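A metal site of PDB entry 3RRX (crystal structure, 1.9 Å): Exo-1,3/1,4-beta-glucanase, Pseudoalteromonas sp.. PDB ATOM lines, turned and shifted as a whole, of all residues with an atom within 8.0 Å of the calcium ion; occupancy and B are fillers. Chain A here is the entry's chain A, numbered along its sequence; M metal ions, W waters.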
ATOM      1  N   VAL A 166      15.635  18.409  10.086  1.00  0.00           N
ATOM      2  CA  VAL A 166      16.291  17.142  10.359  1.00  0.00           C
ATOM      3  C   VAL A 166      16.559  16.955  11.846  1.00  0.00           C
ATOM      4  O   VAL A 166      17.191  17.799  12.477  1.00  0.00           O
ATOM      5  CB  VAL A 166      17.589  17.017   9.534  1.00  0.00           C
ATOM      6  CG1 VAL A 166      18.369  15.759   9.923  1.00  0.00           C
ATOM      7  CG2 VAL A 166      17.238  17.001   8.038  1.00  0.00           C
ATOM      8  N   ARG A 167      16.081  15.828  12.378  1.00  0.00           N
ATOM      9  CA  ARG A 167      16.104  15.548  13.803  1.00  0.00           C
ATOM     10  C   ARG A 167      17.090  14.449  14.201  1.00  0.00           C
ATOM     11  O   ARG A 167      17.375  14.260  15.387  1.00  0.00           O
ATOM     12  CB  ARG A 167      14.695  15.179  14.280  1.00  0.00           C
ATOM     13  CG  ARG A 167      13.623  16.178  13.836  1.00  0.00           C
ATOM     14  CD  ARG A 167      13.792  17.519  14.538  1.00  0.00           C
ATOM     15  NE  ARG A 167      13.331  17.447  15.919  1.00  0.00           N
ATOM     16  CZ  ARG A 167      13.287  18.489  16.746  1.00  0.00           C
ATOM     17  NH1 ARG A 167      13.702  19.678  16.339  1.00  0.00           N
ATOM     18  NH2 ARG A 167      12.830  18.321  17.986  1.00  0.00           N
ATOM     19  N   ASP A 168      17.628  13.728  13.221  1.00  0.00           N
ATOM     20  CA  ASP A 168      18.605  12.667  13.475  1.00  0.00           C
ATOM     21  C   ASP A 168      19.661  12.736  12.372  1.00  0.00           C
ATOM     22  O   ASP A 168      19.376  12.442  11.209  1.00  0.00           O
ATOM     23  CB  ASP A 168      17.918  11.292  13.478  1.00  0.00           C
ATOM     24  CG  ASP A 168      18.835  10.160  13.965  1.00  0.00           C
ATOM     25  OD1 ASP A 168      20.053  10.159  13.651  1.00  0.00           O
ATOM     26  OD2 ASP A 168      18.333   9.265  14.673  1.00  0.00           O
ATOM     27  N   ASP A 169      20.874  13.152  12.739  1.00  0.00           N
ATOM     28  CA  ASP A 169      21.927  13.457  11.759  1.00  0.00           C
ATOM     29  C   ASP A 169      22.504  12.232  11.073  1.00  0.00           C
ATOM     30  O   ASP A 169      23.340  12.361  10.186  1.00  0.00           O
ATOM     31  CB  ASP A 169      23.054  14.278  12.401  1.00  0.00           C
ATOM     32  CG  ASP A 169      22.589  15.626  12.890  1.00  0.00           C
ATOM     33  OD1 ASP A 169      21.507  16.065  12.453  1.00  0.00           O
ATOM     34  OD2 ASP A 169      23.301  16.240  13.715  1.00  0.00           O
ATOM     35  N   THR A 174      20.954  14.935   5.513  1.00  0.00           N
ATOM     36  CA  THR A 174      20.985  15.988   6.525  1.00  0.00           C
ATOM     37  C   THR A 174      21.472  17.355   5.988  1.00  0.00           C
ATOM     38  O   THR A 174      20.928  18.407   6.351  1.00  0.00           O
ATOM     39  CB  THR A 174      21.861  15.547   7.718  1.00  0.00           C
ATOM     40  OG1 THR A 174      21.243  14.415   8.355  1.00  0.00           O
ATOM     41  CG2 THR A 174      22.012  16.664   8.717  1.00  0.00           C
ATOM     42  N   SER A 179      18.321  23.420   9.008  1.00  0.00           N
ATOM     43  CA  SER A 179      18.359  23.398  10.475  1.00  0.00           C
ATOM     44  C   SER A 179      17.558  22.255  11.089  1.00  0.00           C
ATOM     45  O   SER A 179      16.604  21.741  10.489  1.00  0.00           O
ATOM     46  CB  SER A 179      17.820  24.734  11.016  1.00  0.00           C
ATOM     47  OG  SER A 179      17.885  24.797  12.438  1.00  0.00           O
ATOM     48  N   GLU A 180      17.937  21.860  12.301  1.00  0.00           N
ATOM     49  CA  GLU A 180      17.107  20.975  13.112  1.00  0.00           C
ATOM     50  C   GLU A 180      15.902  21.737  13.677  1.00  0.00           C
ATOM     51  O   GLU A 180      14.955  21.137  14.168  1.00  0.00           O
ATOM     52  CB  GLU A 180      17.935  20.414  14.293  1.00  0.00           C
ATOM     53  CG  GLU A 180      18.319  21.472  15.342  1.00  0.00           C
ATOM     54  CD  GLU A 180      19.326  20.963  16.391  1.00  0.00           C
ATOM     55  OE1 GLU A 180      20.141  20.066  16.085  1.00  0.00           O
ATOM     56  OE2 GLU A 180      19.337  21.487  17.524  1.00  0.00           O
ATOM     57  N   ASP A 181      15.963  23.056  13.620  1.00  0.00           N
ATOM     58  CA  ASP A 181      14.961  23.947  14.232  1.00  0.00           C
ATOM     59  C   ASP A 181      13.895  24.390  13.237  1.00  0.00           C
ATOM     60  O   ASP A 181      14.207  25.061  12.257  1.00  0.00           O
ATOM     61  CB  ASP A 181      15.688  25.198  14.765  1.00  0.00           C
ATOM     62  CG  ASP A 181      14.726  26.267  15.329  1.00  0.00           C
ATOM     63  OD1 ASP A 181      13.576  25.927  15.677  1.00  0.00           O
ATOM     64  OD2 ASP A 181      15.144  27.439  15.446  1.00  0.00           O
ATOM     65  N   PRO A 534      26.992  17.806  11.858  1.00  0.00           N
ATOM     66  CA  PRO A 534      27.903  17.631  12.985  1.00  0.00           C
ATOM     67  C   PRO A 534      28.233  16.162  13.109  1.00  0.00           C
ATOM     68  O   PRO A 534      27.375  15.330  12.796  1.00  0.00           O
ATOM     69  CB  PRO A 534      27.065  18.066  14.199  1.00  0.00           C
ATOM     70  CG  PRO A 534      25.982  18.936  13.623  1.00  0.00           C
ATOM     71  CD  PRO A 534      25.674  18.319  12.279  1.00  0.00           C
ATOM     72  N   SER A 581      23.326  25.748  13.358  1.00  0.00           N
ATOM     73  CA  SER A 581      21.909  25.474  13.132  1.00  0.00           C
ATOM     74  C   SER A 581      21.535  24.015  13.424  1.00  0.00           C
ATOM     75  O   SER A 581      20.377  23.636  13.302  1.00  0.00           O
ATOM     76  CB  SER A 581      21.491  25.838  11.692  1.00  0.00           C
ATOM     77  OG  SER A 581      22.116  24.978  10.759  1.00  0.00           O
ATOM     78  N   PHE A 582      22.542  23.226  13.786  1.00  0.00           N
ATOM     79  CA  PHE A 582      22.362  21.845  14.273  1.00  0.00           C
ATOM     80  C   PHE A 582      23.200  21.715  15.547  1.00  0.00           C
ATOM     81  O   PHE A 582      24.317  22.228  15.600  1.00  0.00           O
ATOM     82  CB  PHE A 582      22.871  20.820  13.233  1.00  0.00           C
ATOM     83  CG  PHE A 582      21.941  20.616  12.054  1.00  0.00           C
ATOM     84  CD1 PHE A 582      21.100  19.506  12.007  1.00  0.00           C
ATOM     85  CD2 PHE A 582      21.915  21.526  11.021  1.00  0.00           C
ATOM     86  CE1 PHE A 582      20.232  19.315  10.928  1.00  0.00           C
ATOM     87  CE2 PHE A 582      21.065  21.346   9.937  1.00  0.00           C
ATOM     88  CZ  PHE A 582      20.220  20.239   9.881  1.00  0.00           C
ATOM     89  N   SER A 583      22.671  21.031  16.551  1.00  0.00           N
ATOM     90  CA  SER A 583      23.424  20.849  17.792  1.00  0.00           C
ATOM     91  C   SER A 583      24.608  19.913  17.606  1.00  0.00           C
ATOM     92  O   SER A 583      24.491  18.905  16.893  1.00  0.00           O
ATOM     93  CB  SER A 583      22.509  20.293  18.890  1.00  0.00           C
ATOM     94  OG  SER A 583      21.406  21.153  19.121  1.00  0.00           O
ATOM     95  N   TRP A 584      25.731  20.215  18.252  1.00  0.00           N
ATOM     96  CA  TRP A 584      26.949  19.414  18.100  1.00  0.00           C
ATOM     97  C   TRP A 584      27.114  18.444  19.270  1.00  0.00           C
ATOM     98  O   TRP A 584      27.084  18.857  20.436  1.00  0.00           O
ATOM     99  CB  TRP A 584      28.181  20.329  17.998  1.00  0.00           C
ATOM    100  CG  TRP A 584      29.325  19.663  17.307  1.00  0.00           C
ATOM    101  CD1 TRP A 584      30.188  18.737  17.841  1.00  0.00           C
ATOM    102  CD2 TRP A 584      29.730  19.864  15.953  1.00  0.00           C
ATOM    103  NE1 TRP A 584      31.113  18.351  16.896  1.00  0.00           N
ATOM    104  CE2 TRP A 584      30.843  19.023  15.723  1.00  0.00           C
ATOM    105  CE3 TRP A 584      29.262  20.671  14.906  1.00  0.00           C
ATOM    106  CZ2 TRP A 584      31.498  18.978  14.495  1.00  0.00           C
ATOM    107  CZ3 TRP A 584      29.902  20.622  13.695  1.00  0.00           C
ATOM    108  CH2 TRP A 584      31.005  19.775  13.490  1.00  0.00           C
ATOM    109  N   PRO A 585      27.283  17.144  18.970  1.00  0.00           N
ATOM    110  CA  PRO A 585      27.283  16.085  19.985  1.00  0.00           C
ATOM    111  C   PRO A 585      28.558  16.018  20.835  1.00  0.00           C
ATOM    112  O   PRO A 585      29.654  16.217  20.325  1.00  0.00           O
ATOM    113  CB  PRO A 585      27.141  14.809  19.154  1.00  0.00           C
ATOM    114  CG  PRO A 585      27.815  15.173  17.827  1.00  0.00           C
ATOM    115  CD  PRO A 585      27.418  16.606  17.610  1.00  0.00           C
ATOM    116  N   GLN A 590      24.924  10.351  20.876  1.00  0.00           N
ATOM    117  CA  GLN A 590      23.882  11.369  20.977  1.00  0.00           C
ATOM    118  C   GLN A 590      23.180  11.579  19.631  1.00  0.00           C
ATOM    119  O   GLN A 590      23.375  12.601  18.970  1.00  0.00           O
ATOM    120  CB  GLN A 590      24.470  12.690  21.455  1.00  0.00           C
ATOM    121  CG  GLN A 590      24.605  12.804  22.950  1.00  0.00           C
ATOM    122  CD  GLN A 590      25.139  14.149  23.379  1.00  0.00           C
ATOM    123  OE1 GLN A 590      26.050  14.690  22.764  1.00  0.00           O
ATOM    124  NE2 GLN A 590      24.563  14.703  24.442  1.00  0.00           N
ATOM    125  N   PHE A 591      22.361  10.599  19.249  1.00  0.00           N
ATOM    126  CA  PHE A 591      21.812  10.538  17.896  1.00  0.00           C
ATOM    127  C   PHE A 591      20.702  11.542  17.594  1.00  0.00           C
ATOM    128  O   PHE A 591      20.534  11.965  16.454  1.00  0.00           O
ATOM    129  CB  PHE A 591      21.297   9.127  17.598  1.00  0.00           C
ATOM    130  CG  PHE A 591      22.357   8.090  17.642  1.00  0.00           C
ATOM    131  CD1 PHE A 591      23.401   8.116  16.735  1.00  0.00           C
ATOM    132  CD2 PHE A 591      22.318   7.078  18.598  1.00  0.00           C
ATOM    133  CE1 PHE A 591      24.401   7.153  16.780  1.00  0.00           C
ATOM    134  CE2 PHE A 591      23.305   6.116  18.638  1.00  0.00           C
ATOM    135  CZ  PHE A 591      24.349   6.152  17.734  1.00  0.00           C
ATOM    136  N   THR A 592      19.912  11.880  18.591  1.00  0.00           N
ATOM    137  CA  THR A 592      18.816  12.825  18.390  1.00  0.00           C
ATOM    138  C   THR A 592      18.941  13.964  19.384  1.00  0.00           C
ATOM    139  O   THR A 592      18.131  14.109  20.291  1.00  0.00           O
ATOM    140  CB  THR A 592      17.441  12.139  18.539  1.00  0.00           C
ATOM    141  OG1 THR A 592      17.410  11.398  19.758  1.00  0.00           O
ATOM    142  CG2 THR A 592      17.189  11.196  17.363  1.00  0.00           C
ATOM    143  N   LEU A 593      19.973  14.771  19.196  1.00  0.00           N
ATOM    144  CA  LEU A 593      20.281  15.876  20.075  1.00  0.00           C
ATOM    145  C   LEU A 593      19.694  17.124  19.440  1.00  0.00           C
ATOM    146  O   LEU A 593      20.255  17.612  18.469  1.00  0.00           O
ATOM    147  CB  LEU A 593      21.797  16.015  20.142  1.00  0.00           C
ATOM    148  CG  LEU A 593      22.429  17.154  20.944  1.00  0.00           C
ATOM    149  CD1 LEU A 593      22.204  16.943  22.441  1.00  0.00           C
ATOM    150  CD2 LEU A 593      23.905  17.224  20.614  1.00  0.00           C
ATOM    151  N   ASN A 594      18.599  17.652  19.982  1.00  0.00           N
ATOM    152  CA  ASN A 594      17.921  18.803  19.371  1.00  0.00           C
ATOM    153  C   ASN A 594      17.575  19.904  20.349  1.00  0.00           C
ATOM    154  O   ASN A 594      17.262  19.628  21.517  1.00  0.00           O
ATOM    155  CB  ASN A 594      16.649  18.330  18.642  1.00  0.00           C
ATOM    156  CG  ASN A 594      16.956  17.387  17.500  1.00  0.00           C
ATOM    157  OD1 ASN A 594      17.710  17.739  16.598  1.00  0.00           O
ATOM    158  ND2 ASN A 594      16.402  16.184  17.548  1.00  0.00           N
ATOM    159  N   LEU A 595      17.619  21.153  19.897  1.00  0.00           N
ATOM    160  CA  LEU A 595      17.318  22.268  20.779  1.00  0.00           C
ATOM    161  C   LEU A 595      15.910  22.080  21.351  1.00  0.00           C
ATOM    162  O   LEU A 595      15.031  21.530  20.686  1.00  0.00           O
ATOM    163  CB  LEU A 595      17.429  23.604  20.039  1.00  0.00           C
ATOM    164  CG  LEU A 595      16.150  24.116  19.383  1.00  0.00           C
ATOM    165  CD1 LEU A 595      16.343  25.537  18.856  1.00  0.00           C
ATOM    166  CD2 LEU A 595      15.716  23.171  18.264  1.00  0.00           C
ATOM    167  N   ASP A 597      15.137  19.995  23.542  1.00  0.00           N
ATOM    168  CA  ASP A 597      15.030  18.668  24.136  1.00  0.00           C
ATOM    169  C   ASP A 597      14.971  18.778  25.660  1.00  0.00           C
ATOM    170  O   ASP A 597      15.583  19.672  26.257  1.00  0.00           O
ATOM    171  CB  ASP A 597      16.213  17.781  23.727  1.00  0.00           C
ATOM    172  CG  ASP A 597      16.016  17.102  22.374  1.00  0.00           C
ATOM    173  OD1 ASP A 597      14.949  17.294  21.738  1.00  0.00           O
ATOM    174  OD2 ASP A 597      16.922  16.348  21.955  1.00  0.00           O
ATOM    175  N   TYR A 600      19.045  18.178  27.445  1.00  0.00           N
ATOM    176  CA  TYR A 600      19.840  18.786  26.358  1.00  0.00           C
ATOM    177  C   TYR A 600      21.264  19.042  26.802  1.00  0.00           C
ATOM    178  O   TYR A 600      21.525  20.033  27.491  1.00  0.00           O
ATOM    179  CB  TYR A 600      19.179  20.093  25.896  1.00  0.00           C
ATOM    180  CG  TYR A 600      19.799  20.724  24.657  1.00  0.00           C
ATOM    181  CD1 TYR A 600      20.293  22.019  24.695  1.00  0.00           C
ATOM    182  CD2 TYR A 600      19.883  20.020  23.454  1.00  0.00           C
ATOM    183  CE1 TYR A 600      20.852  22.613  23.562  1.00  0.00           C
ATOM    184  CE2 TYR A 600      20.452  20.605  22.314  1.00  0.00           C
ATOM    185  CZ  TYR A 600      20.936  21.893  22.378  1.00  0.00           C
ATOM    186  OH  TYR A 600      21.498  22.488  21.278  1.00  0.00           O
ATOM    187  N   TYR A 606      23.005  24.581  19.700  1.00  0.00           N
ATOM    188  CA  TYR A 606      22.356  25.370  18.660  1.00  0.00           C
ATOM    189  C   TYR A 606      22.598  26.829  18.991  1.00  0.00           C
ATOM    190  O   TYR A 606      22.408  27.250  20.139  1.00  0.00           O
ATOM    191  CB  TYR A 606      20.854  25.085  18.672  1.00  0.00           C
ATOM    192  CG  TYR A 606      20.042  25.893  17.687  1.00  0.00           C
ATOM    193  CD1 TYR A 606      19.765  25.400  16.421  1.00  0.00           C
ATOM    194  CD2 TYR A 606      19.533  27.149  18.024  1.00  0.00           C
ATOM    195  CE1 TYR A 606      19.004  26.124  15.514  1.00  0.00           C
ATOM    196  CE2 TYR A 606      18.776  27.880  17.129  1.00  0.00           C
ATOM    197  CZ  TYR A 606      18.516  27.363  15.871  1.00  0.00           C
ATOM    198  OH  TYR A 606      17.768  28.095  14.972  1.00  0.00           O
HETATM  199 CA    CA M   1      20.061  17.732  16.106  1.00  0.00          CA
HETATM  200  O   HOH W   1      22.423  17.752  15.516  1.00  0.00           O
HETATM  201  O   HOH W   2      19.466  17.129  13.844  1.00  0.00           O
HETATM  202  O   HOH W   3      20.181  15.213  16.224  1.00  0.00           O
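The side-chain amide nitrogen (ND2) of Asn 594 lies within hydrogen-bond range of the backbone carbonyl oxygen (O) of Arg 167.
N of Asn 594 sits at hydrogen-bond distance from OD2 of Asp 597.
The guanidinium group (NH1) of Arg 167 is in hydrogen-bond range of the backbone carbonyl oxygen (O) of Glu 180 (2.9 Å).
The backbone NH of Glu 180 lies within hydrogen-bond range of the backbone carbonyl oxygen of Ser 581 (3.2 Å).
OE2 of Glu 180 sits at hydrogen-bond distance from N of Leu 595 (2.9 Å).
OE2 of Glu 180 lies within hydrogen-bond range of OG of Ser 583 (2.6 Å).
Along chain A the residues within 4 Å of the calcium ion span positions 180 to 594.
The calcium ion is bound by the side-chain carboxylate of Glu 180 (2.3 Å), the backbone carbonyl oxygen of Leu 593 (2.4 Å), the side-chain amide oxygen of Asn 594 (2.4 Å), water W2 (2.4 Å), water W1 (2.4 Å) and water W3 (2.5 Å).
Water W3 lies within hydrogen-bond range of N of Leu 593 (3.0 Å), O of Arg 167 (3.1 Å) and O of Phe 591 (3.3 Å).
Water W1 lies within hydrogen-bond range of the side-chain carboxylate (OD2) of Asp 169 (2.5 Å) and the backbone carbonyl oxygen (O) of Ser 583 (2.7 Å).
Water W2 bridges the side-chain carboxylate (OD1) of Asp 169 and the backbone carbonyl oxygen (O) of Val 166.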
